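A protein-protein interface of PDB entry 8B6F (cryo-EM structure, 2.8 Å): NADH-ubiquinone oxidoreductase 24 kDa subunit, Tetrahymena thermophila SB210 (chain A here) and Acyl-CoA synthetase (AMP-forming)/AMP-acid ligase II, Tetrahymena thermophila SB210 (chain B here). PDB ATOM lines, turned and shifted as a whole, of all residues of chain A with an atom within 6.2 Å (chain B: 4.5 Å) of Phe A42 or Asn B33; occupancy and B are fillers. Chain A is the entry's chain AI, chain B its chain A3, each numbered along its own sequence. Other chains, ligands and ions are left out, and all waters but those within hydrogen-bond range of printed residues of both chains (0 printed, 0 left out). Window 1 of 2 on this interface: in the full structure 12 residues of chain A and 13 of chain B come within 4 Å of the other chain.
The side-chain amino group of Lys A90 sits at hydrogen-bond distance from the side-chain amide oxygen of Asn B33, at 3.1 Å.
The side-chain amino group (NZ) of Lys A93 sits at hydrogen-bond distance from the backbone carbonyl oxygen (O) of Thr B43 (3.1 Å).
The side-chain amino group (NZ) of Lys A90 lies within hydrogen-bond range of the backbone carbonyl oxygen (O) of Asn B31 (2.6 Å).
OE1 of Glu A43 sits close to ND2 of Asn B33.
The side-chain hydroxyl of Thr B43 sits at hydrogen-bond distance from the backbone carbonyl oxygen of Val B35, 3.4 Å away.
The side-chain hydroxyl of Tyr A49 lies within hydrogen-bond range of the side-chain carboxylate of Glu A43, at 2.5 Å.
The backbone carbonyl oxygen of Glu A43 is in hydrogen-bond range of the side-chain amide nitrogen of Gln A78 (2.5 Å).
O of Arg B32 lies close to N of Phe B46, at 3.3 Å.
O of Phe A42 touches ND2 of Asn B33 (3.6 Å).
Glu A43 touches Arg B32 (OE2 to CG, 3.2 Å).
OH of Tyr A49 touches O of Asn B31, 3.7 Å away.
Tyr A49 touches Arg B32 (OH to CA, 3.4 Å).
Thr B45 touches Lys A90 (CG2 to NZ, 3.3 Å).
CG2 of Thr B45 touches CD of Lys A93, at 3.7 Å.
Of chain B, only Asn B33 (3.6 Å) comes within 4 Å of Phe A42.
Asn B33 touches just these residues of chain A: Phe A42, Glu A43 and Lys A90.
Printed residues of chain A within 4 Å of Thr B43: Lys A93 (3.1 Å).
Of the printed residues of chain B, Lys A93 touches Thr B43 (3.1 Å) and Thr B45 (3.7 Å).
Of the printed residues of chain A, Arg B32 touches Glu A43 and Tyr A49.
Of the printed residues of chain B, Tyr A49 touches Asn B31 (3.7 Å) and Arg B32 (3.4 Å).
Printed residues of chain B within 4 Å of Glu A43: Arg B32 and Asn B33.
Ser A86 touches none of the printed residues of chain B.
Hydrophobic or aromatic side chains of chain A within 4 Å of the printed part of chain B: Tyr A49.
Among the printed residues, no Asp or Glu carboxylate lies within 4 Å of a Lys or Arg side-chain nitrogen of the other chain.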
ATOM      1  N   VAL A  40     -24.200  -6.168   0.957  1.00  0.00           N
ATOM      2  CA  VAL A  40     -24.048  -5.026   1.866  1.00  0.00           C
ATOM      3  C   VAL A  40     -23.853  -5.544   3.288  1.00  0.00           C
ATOM      4  O   VAL A  40     -24.677  -6.340   3.770  1.00  0.00           O
ATOM      5  CB  VAL A  40     -25.268  -4.107   1.776  1.00  0.00           C
ATOM      6  CG1 VAL A  40     -25.103  -2.908   2.700  1.00  0.00           C
ATOM      7  CG2 VAL A  40     -25.487  -3.645   0.342  1.00  0.00           C
ATOM      8  N   PRO A  41     -22.801  -5.136   3.993  1.00  0.00           N
ATOM      9  CA  PRO A  41     -22.588  -5.634   5.355  1.00  0.00           C
ATOM     10  C   PRO A  41     -23.443  -4.896   6.373  1.00  0.00           C
ATOM     11  O   PRO A  41     -23.969  -3.810   6.126  1.00  0.00           O
ATOM     12  CB  PRO A  41     -21.100  -5.365   5.595  1.00  0.00           C
ATOM     13  CG  PRO A  41     -20.821  -4.156   4.783  1.00  0.00           C
ATOM     14  CD  PRO A  41     -21.706  -4.247   3.564  1.00  0.00           C
ATOM     15  N   PHE A  42     -23.570  -5.518   7.542  1.00  0.00           N
ATOM     16  CA  PHE A  42     -24.251  -4.895   8.667  1.00  0.00           C
ATOM     17  C   PHE A  42     -23.851  -5.622   9.939  1.00  0.00           C
ATOM     18  O   PHE A  42     -23.938  -6.852  10.003  1.00  0.00           O
ATOM     19  CB  PHE A  42     -25.770  -4.927   8.494  1.00  0.00           C
ATOM     20  CG  PHE A  42     -26.510  -4.340   9.654  1.00  0.00           C
ATOM     21  CD1 PHE A  42     -26.691  -2.971   9.750  1.00  0.00           C
ATOM     22  CD2 PHE A  42     -27.012  -5.150  10.656  1.00  0.00           C
ATOM     23  CE1 PHE A  42     -27.364  -2.423  10.817  1.00  0.00           C
ATOM     24  CE2 PHE A  42     -27.684  -4.608  11.728  1.00  0.00           C
ATOM     25  CZ  PHE A  42     -27.859  -3.241  11.807  1.00  0.00           C
ATOM     26  N   GLU A  43     -23.417  -4.864  10.944  1.00  0.00           N
ATOM     27  CA  GLU A  43     -23.014  -5.430  12.223  1.00  0.00           C
ATOM     28  C   GLU A  43     -23.476  -4.513  13.344  1.00  0.00           C
ATOM     29  O   GLU A  43     -23.223  -3.306  13.306  1.00  0.00           O
ATOM     30  CB  GLU A  43     -21.492  -5.620  12.284  1.00  0.00           C
ATOM     31  CG  GLU A  43     -20.982  -6.146  13.616  1.00  0.00           C
ATOM     32  CD  GLU A  43     -21.635  -7.453  14.015  1.00  0.00           C
ATOM     33  OE1 GLU A  43     -22.142  -8.164  13.124  1.00  0.00           O
ATOM     34  OE2 GLU A  43     -21.646  -7.768  15.222  1.00  0.00           O
ATOM     35  N   PHE A  44     -24.149  -5.089  14.336  1.00  0.00           N
ATOM     36  CA  PHE A  44     -24.584  -4.315  15.489  1.00  0.00           C
ATOM     37  C   PHE A  44     -23.384  -3.860  16.310  1.00  0.00           C
ATOM     38  O   PHE A  44     -22.417  -4.603  16.493  1.00  0.00           O
ATOM     39  CB  PHE A  44     -25.524  -5.144  16.366  1.00  0.00           C
ATOM     40  CG  PHE A  44     -26.869  -5.395  15.749  1.00  0.00           C
ATOM     41  CD1 PHE A  44     -27.884  -4.463  15.869  1.00  0.00           C
ATOM     42  CD2 PHE A  44     -27.122  -6.571  15.065  1.00  0.00           C
ATOM     43  CE1 PHE A  44     -29.126  -4.693  15.308  1.00  0.00           C
ATOM     44  CE2 PHE A  44     -28.362  -6.809  14.502  1.00  0.00           C
ATOM     45  CZ  PHE A  44     -29.365  -5.868  14.624  1.00  0.00           C
ATOM     46  N   TYR A  49     -25.792  -4.559  20.910  1.00  0.00           N
ATOM     47  CA  TYR A  49     -25.818  -5.918  21.437  1.00  0.00           C
ATOM     48  C   TYR A  49     -26.292  -5.936  22.885  1.00  0.00           C
ATOM     49  O   TYR A  49     -27.068  -6.813  23.281  1.00  0.00           O
ATOM     50  CB  TYR A  49     -24.434  -6.557  21.317  1.00  0.00           C
ATOM     51  CG  TYR A  49     -24.191  -7.215  19.979  1.00  0.00           C
ATOM     52  CD1 TYR A  49     -24.845  -8.390  19.634  1.00  0.00           C
ATOM     53  CD2 TYR A  49     -23.302  -6.664  19.065  1.00  0.00           C
ATOM     54  CE1 TYR A  49     -24.626  -8.996  18.413  1.00  0.00           C
ATOM     55  CE2 TYR A  49     -23.076  -7.264  17.841  1.00  0.00           C
ATOM     56  CZ  TYR A  49     -23.741  -8.429  17.522  1.00  0.00           C
ATOM     57  OH  TYR A  49     -23.521  -9.033  16.306  1.00  0.00           O
ATOM     58  N   LEU A  74     -33.683  -0.841  16.475  1.00  0.00           N
ATOM     59  CA  LEU A  74     -32.254  -0.662  16.703  1.00  0.00           C
ATOM     60  C   LEU A  74     -31.495  -0.564  15.385  1.00  0.00           C
ATOM     61  O   LEU A  74     -30.574   0.249  15.250  1.00  0.00           O
ATOM     62  CB  LEU A  74     -31.710  -1.813  17.549  1.00  0.00           C
ATOM     63  CG  LEU A  74     -32.209  -1.908  18.995  1.00  0.00           C
ATOM     64  CD1 LEU A  74     -31.548  -3.072  19.715  1.00  0.00           C
ATOM     65  CD2 LEU A  74     -31.977  -0.609  19.747  1.00  0.00           C
ATOM     66  N   VAL A  75     -31.866  -1.384  14.401  1.00  0.00           N
ATOM     67  CA  VAL A  75     -31.213  -1.321  13.097  1.00  0.00           C
ATOM     68  C   VAL A  75     -31.428   0.045  12.459  1.00  0.00           C
ATOM     69  O   VAL A  75     -30.495   0.642  11.907  1.00  0.00           O
ATOM     70  CB  VAL A  75     -31.701  -2.459  12.184  1.00  0.00           C
ATOM     71  CG1 VAL A  75     -31.281  -2.218  10.737  1.00  0.00           C
ATOM     72  CG2 VAL A  75     -31.165  -3.777  12.671  1.00  0.00           C
ATOM     73  N   GLN A  76     -32.656   0.561  12.519  1.00  0.00           N
ATOM     74  CA  GLN A  76     -32.921   1.878  11.954  1.00  0.00           C
ATOM     75  C   GLN A  76     -32.108   2.948  12.669  1.00  0.00           C
ATOM     76  O   GLN A  76     -31.552   3.846  12.028  1.00  0.00           O
ATOM     77  CB  GLN A  76     -34.413   2.199  12.042  1.00  0.00           C
ATOM     78  CG  GLN A  76     -35.253   1.532  10.971  1.00  0.00           C
ATOM     79  CD  GLN A  76     -36.615   2.178  10.823  1.00  0.00           C
ATOM     80  OE1 GLN A  76     -37.082   2.416   9.711  1.00  0.00           O
ATOM     81  NE2 GLN A  76     -37.264   2.459  11.948  1.00  0.00           N
ATOM     82  N   GLN A  78     -29.235   2.565  14.200  1.00  0.00           N
ATOM     83  CA  GLN A  78     -27.827   2.408  13.853  1.00  0.00           C
ATOM     84  C   GLN A  78     -27.547   2.877  12.430  1.00  0.00           C
ATOM     85  O   GLN A  78     -26.516   3.507  12.170  1.00  0.00           O
ATOM     86  CB  GLN A  78     -27.408   0.949  14.030  1.00  0.00           C
ATOM     87  CG  GLN A  78     -25.937   0.690  13.759  1.00  0.00           C
ATOM     88  CD  GLN A  78     -25.535  -0.733  14.081  1.00  0.00           C
ATOM     89  OE1 GLN A  78     -26.323  -1.502  14.630  1.00  0.00           O
ATOM     90  NE2 GLN A  78     -24.304  -1.093  13.738  1.00  0.00           N
ATOM     91  N   ASN A  79     -28.446   2.575  11.498  1.00  0.00           N
ATOM     92  CA  ASN A  79     -28.254   2.915  10.097  1.00  0.00           C
ATOM     93  C   ASN A  79     -28.809   4.316   9.834  1.00  0.00           C
ATOM     94  O   ASN A  79     -29.155   5.055  10.759  1.00  0.00           O
ATOM     95  CB  ASN A  79     -28.915   1.858   9.215  1.00  0.00           C
ATOM     96  CG  ASN A  79     -28.251   1.730   7.861  1.00  0.00           C
ATOM     97  OD1 ASN A  79     -28.505   2.522   6.956  1.00  0.00           O
ATOM     98  ND2 ASN A  79     -27.397   0.724   7.713  1.00  0.00           N
ATOM     99  N   PRO A  84     -31.533  -2.386   6.129  1.00  0.00           N
ATOM    100  CA  PRO A  84     -31.027  -3.156   4.986  1.00  0.00           C
ATOM    101  C   PRO A  84     -31.453  -4.615   5.045  1.00  0.00           C
ATOM    102  O   PRO A  84     -31.728  -5.173   6.109  1.00  0.00           O
ATOM    103  CB  PRO A  84     -29.503  -3.022   5.104  1.00  0.00           C
ATOM    104  CG  PRO A  84     -29.281  -1.844   5.984  1.00  0.00           C
ATOM    105  CD  PRO A  84     -30.434  -1.822   6.932  1.00  0.00           C
ATOM    106  N   SER A  86     -29.532  -7.138   4.482  1.00  0.00           N
ATOM    107  CA  SER A  86     -28.521  -7.842   5.264  1.00  0.00           C
ATOM    108  C   SER A  86     -28.802  -7.722   6.755  1.00  0.00           C
ATOM    109  O   SER A  86     -28.649  -8.693   7.504  1.00  0.00           O
ATOM    110  CB  SER A  86     -27.132  -7.302   4.930  1.00  0.00           C
ATOM    111  OG  SER A  86     -27.045  -5.913   5.192  1.00  0.00           O
ATOM    112  N   ALA A  87     -29.217  -6.538   7.204  1.00  0.00           N
ATOM    113  CA  ALA A  87     -29.569  -6.361   8.608  1.00  0.00           C
ATOM    114  C   ALA A  87     -30.757  -7.232   8.990  1.00  0.00           C
ATOM    115  O   ALA A  87     -30.784  -7.815  10.079  1.00  0.00           O
ATOM    116  CB  ALA A  87     -29.873  -4.891   8.892  1.00  0.00           C
ATOM    117  N   MET A  88     -31.751  -7.332   8.107  1.00  0.00           N
ATOM    118  CA  MET A  88     -32.901  -8.186   8.386  1.00  0.00           C
ATOM    119  C   MET A  88     -32.474  -9.643   8.516  1.00  0.00           C
ATOM    120  O   MET A  88     -32.936 -10.356   9.414  1.00  0.00           O
ATOM    121  CB  MET A  88     -33.948  -8.021   7.284  1.00  0.00           C
ATOM    122  CG  MET A  88     -34.427  -6.582   7.129  1.00  0.00           C
ATOM    123  SD  MET A  88     -35.208  -6.237   5.545  1.00  0.00           S
ATOM    124  CE  MET A  88     -36.739  -7.125   5.762  1.00  0.00           C
ATOM    125  N   LYS A  90     -29.503 -10.697   9.394  1.00  0.00           N
ATOM    126  CA  LYS A  90     -28.761 -10.800  10.647  1.00  0.00           C
ATOM    127  C   LYS A  90     -29.709 -10.905  11.835  1.00  0.00           C
ATOM    128  O   LYS A  90     -29.483 -11.707  12.748  1.00  0.00           O
ATOM    129  CB  LYS A  90     -27.831  -9.594  10.800  1.00  0.00           C
ATOM    130  CG  LYS A  90     -26.986  -9.597  12.067  1.00  0.00           C
ATOM    131  CD  LYS A  90     -26.040 -10.789  12.107  1.00  0.00           C
ATOM    132  CE  LYS A  90     -25.122 -10.722  13.316  1.00  0.00           C
ATOM    133  NZ  LYS A  90     -24.212 -11.899  13.388  1.00  0.00           N
ATOM    134  N   ILE A  91     -30.781 -10.112  11.839  1.00  0.00           N
ATOM    135  CA  ILE A  91     -31.760 -10.191  12.921  1.00  0.00           C
ATOM    136  C   ILE A  91     -32.383 -11.577  12.970  1.00  0.00           C
ATOM    137  O   ILE A  91     -32.532 -12.170  14.046  1.00  0.00           O
ATOM    138  CB  ILE A  91     -32.843  -9.109  12.754  1.00  0.00           C
ATOM    139  CG1 ILE A  91     -32.261  -7.711  12.924  1.00  0.00           C
ATOM    140  CG2 ILE A  91     -33.975  -9.312  13.760  1.00  0.00           C
ATOM    141  CD1 ILE A  91     -33.193  -6.642  12.422  1.00  0.00           C
ATOM    142  N   LYS A  93     -31.105 -14.403  11.935  1.00  0.00           N
ATOM    143  CA  LYS A  93     -30.119 -15.353  12.438  1.00  0.00           C
ATOM    144  C   LYS A  93     -29.967 -15.238  13.951  1.00  0.00           C
ATOM    145  O   LYS A  93     -29.889 -16.252  14.653  1.00  0.00           O
ATOM    146  CB  LYS A  93     -28.776 -15.124  11.745  1.00  0.00           C
ATOM    147  CG  LYS A  93     -27.709 -16.147  12.112  1.00  0.00           C
ATOM    148  CD  LYS A  93     -26.347 -15.769  11.546  1.00  0.00           C
ATOM    149  CE  LYS A  93     -26.341 -15.798  10.025  1.00  0.00           C
ATOM    150  NZ  LYS A  93     -25.001 -15.454   9.472  1.00  0.00           N
ATOM    151  N   ASN B  31     -22.103 -13.898  18.842  1.00  0.00           N
ATOM    152  CA  ASN B  31     -23.106 -13.514  17.857  1.00  0.00           C
ATOM    153  C   ASN B  31     -22.533 -12.670  16.728  1.00  0.00           C
ATOM    154  O   ASN B  31     -23.117 -12.638  15.639  1.00  0.00           O
ATOM    155  CB  ASN B  31     -24.239 -12.747  18.541  1.00  0.00           C
ATOM    156  CG  ASN B  31     -24.996 -13.597  19.540  1.00  0.00           C
ATOM    157  OD1 ASN B  31     -24.509 -14.637  19.982  1.00  0.00           O
ATOM    158  ND2 ASN B  31     -26.197 -13.160  19.900  1.00  0.00           N
ATOM    159  N   ARG B  32     -21.412 -11.993  16.956  1.00  0.00           N
ATOM    160  CA  ARG B  32     -20.826 -11.144  15.930  1.00  0.00           C
ATOM    161  C   ARG B  32     -20.402 -11.974  14.723  1.00  0.00           C
ATOM    162  O   ARG B  32     -19.963 -13.120  14.851  1.00  0.00           O
ATOM    163  CB  ARG B  32     -19.624 -10.385  16.494  1.00  0.00           C
ATOM    164  CG  ARG B  32     -18.914  -9.505  15.478  1.00  0.00           C
ATOM    165  CD  ARG B  32     -17.800  -8.699  16.122  1.00  0.00           C
ATOM    166  NE  ARG B  32     -17.194  -7.766  15.178  1.00  0.00           N
ATOM    167  CZ  ARG B  32     -16.245  -8.084  14.308  1.00  0.00           C
ATOM    168  NH1 ARG B  32     -15.763  -9.314  14.227  1.00  0.00           N
ATOM    169  NH2 ARG B  32     -15.769  -7.146  13.496  1.00  0.00           N
ATOM    170  N   ASN B  33     -20.539 -11.384  13.540  1.00  0.00           N
ATOM    171  CA  ASN B  33     -20.128 -12.062  12.318  1.00  0.00           C
ATOM    172  C   ASN B  33     -18.634 -12.352  12.351  1.00  0.00           C
ATOM    173  O   ASN B  33     -17.832 -11.527  12.795  1.00  0.00           O
ATOM    174  CB  ASN B  33     -20.473 -11.210  11.097  1.00  0.00           C
ATOM    175  CG  ASN B  33     -21.942 -10.853  11.033  1.00  0.00           C
ATOM    176  OD1 ASN B  33     -22.770 -11.654  10.603  1.00  0.00           O
ATOM    177  ND2 ASN B  33     -22.274  -9.640  11.457  1.00  0.00           N
ATOM    178  N   ALA B  34     -18.260 -13.539  11.877  1.00  0.00           N
ATOM    179  CA  ALA B  34     -16.872 -13.987  11.903  1.00  0.00           C
ATOM    180  C   ALA B  34     -16.174 -13.834  10.558  1.00  0.00           C
ATOM    181  O   ALA B  34     -15.089 -13.251  10.489  1.00  0.00           O
ATOM    182  CB  ALA B  34     -16.805 -15.449  12.357  1.00  0.00           C
ATOM    183  N   VAL B  35     -16.771 -14.349   9.483  1.00  0.00           N
ATOM    184  CA  VAL B  35     -16.136 -14.334   8.171  1.00  0.00           C
ATOM    185  C   VAL B  35     -17.219 -14.294   7.102  1.00  0.00           C
ATOM    186  O   VAL B  35     -18.339 -14.769   7.308  1.00  0.00           O
ATOM    187  CB  VAL B  35     -15.205 -15.555   7.984  1.00  0.00           C
ATOM    188  CG1 VAL B  35     -15.997 -16.855   8.061  1.00  0.00           C
ATOM    189  CG2 VAL B  35     -14.441 -15.460   6.670  1.00  0.00           C
ATOM    190  N   THR B  43     -22.097 -16.033   4.926  1.00  0.00           N
ATOM    191  CA  THR B  43     -21.446 -15.348   6.034  1.00  0.00           C
ATOM    192  C   THR B  43     -21.642 -16.157   7.309  1.00  0.00           C
ATOM    193  O   THR B  43     -22.759 -16.592   7.608  1.00  0.00           O
ATOM    194  CB  THR B  43     -22.002 -13.931   6.209  1.00  0.00           C
ATOM    195  OG1 THR B  43     -21.350 -13.289   7.313  1.00  0.00           O
ATOM    196  CG2 THR B  43     -23.506 -13.955   6.453  1.00  0.00           C
ATOM    197  N   TRP B  44     -20.557 -16.360   8.051  1.00  0.00           N
ATOM    198  CA  TRP B  44     -20.564 -17.174   9.257  1.00  0.00           C
ATOM    199  C   TRP B  44     -20.295 -16.311  10.482  1.00  0.00           C
ATOM    200  O   TRP B  44     -19.403 -15.458  10.470  1.00  0.00           O
ATOM    201  CB  TRP B  44     -19.507 -18.279   9.182  1.00  0.00           C
ATOM    202  CG  TRP B  44     -19.802 -19.356   8.186  1.00  0.00           C
ATOM    203  CD1 TRP B  44     -20.956 -19.532   7.480  1.00  0.00           C
ATOM    204  CD2 TRP B  44     -18.921 -20.411   7.786  1.00  0.00           C
ATOM    205  NE1 TRP B  44     -20.847 -20.632   6.664  1.00  0.00           N
ATOM    206  CE2 TRP B  44     -19.607 -21.189   6.834  1.00  0.00           C
ATOM    207  CE3 TRP B  44     -17.617 -20.771   8.139  1.00  0.00           C
ATOM    208  CZ2 TRP B  44     -19.034 -22.307   6.232  1.00  0.00           C
ATOM    209  CZ3 TRP B  44     -17.049 -21.880   7.543  1.00  0.00           C
ATOM    210  CH2 TRP B  44     -17.757 -22.635   6.599  1.00  0.00           C
ATOM    211  N   THR B  45     -21.072 -16.538  11.536  1.00  0.00           N
ATOM    212  CA  THR B  45     -20.756 -15.978  12.837  1.00  0.00           C
ATOM    213  C   THR B  45     -19.675 -16.821  13.512  1.00  0.00           C
ATOM    214  O   THR B  45     -19.282 -17.883  13.023  1.00  0.00           O
ATOM    215  CB  THR B  45     -22.003 -15.910  13.718  1.00  0.00           C
ATOM    216  OG1 THR B  45     -22.546 -17.225  13.890  1.00  0.00           O
ATOM    217  CG2 THR B  45     -23.053 -15.009  13.090  1.00  0.00           C
ATOM    218  N   PHE B  46     -19.189 -16.335  14.655  1.00  0.00           N
ATOM    219  CA  PHE B  46     -18.162 -17.078  15.377  1.00  0.00           C
ATOM    220  C   PHE B  46     -18.676 -18.445  15.806  1.00  0.00           C
ATOM    221  O   PHE B  46     -17.954 -19.445  15.715  1.00  0.00           O
ATOM    222  CB  PHE B  46     -17.684 -16.274  16.586  1.00  0.00           C
ATOM    223  CG  PHE B  46     -16.857 -15.078  16.223  1.00  0.00           C
ATOM    224  CD1 PHE B  46     -15.514 -15.216  15.919  1.00  0.00           C
ATOM    225  CD2 PHE B  46     -17.421 -13.815  16.185  1.00  0.00           C
ATOM    226  CE1 PHE B  46     -14.748 -14.117  15.583  1.00  0.00           C
ATOM    227  CE2 PHE B  46     -16.662 -12.712  15.850  1.00  0.00           C
ATOM    228  CZ  PHE B  46     -15.323 -12.864  15.548  1.00  0.00           C
ATOM    229  N   TYR B 259     -13.053  -8.910  11.159  1.00  0.00           N
ATOM    230  CA  TYR B 259     -14.005  -9.388  10.160  1.00  0.00           C
ATOM    231  C   TYR B 259     -13.261  -9.603   8.850  1.00  0.00           C
ATOM    232  O   TYR B 259     -12.788  -8.642   8.234  1.00  0.00           O
ATOM    233  CB  TYR B 259     -15.146  -8.390   9.987  1.00  0.00           C
ATOM    234  CG  TYR B 259     -16.268  -8.877   9.104  1.00  0.00           C
ATOM    235  CD1 TYR B 259     -17.168  -9.832   9.556  1.00  0.00           C
ATOM    236  CD2 TYR B 259     -16.443  -8.364   7.828  1.00  0.00           C
ATOM    237  CE1 TYR B 259     -18.203 -10.271   8.756  1.00  0.00           C
ATOM    238  CE2 TYR B 259     -17.474  -8.796   7.020  1.00  0.00           C
ATOM    239  CZ  TYR B 259     -18.351  -9.750   7.490  1.00  0.00           C
ATOM    240  OH  TYR B 259     -19.382 -10.183   6.692  1.00  0.00           O
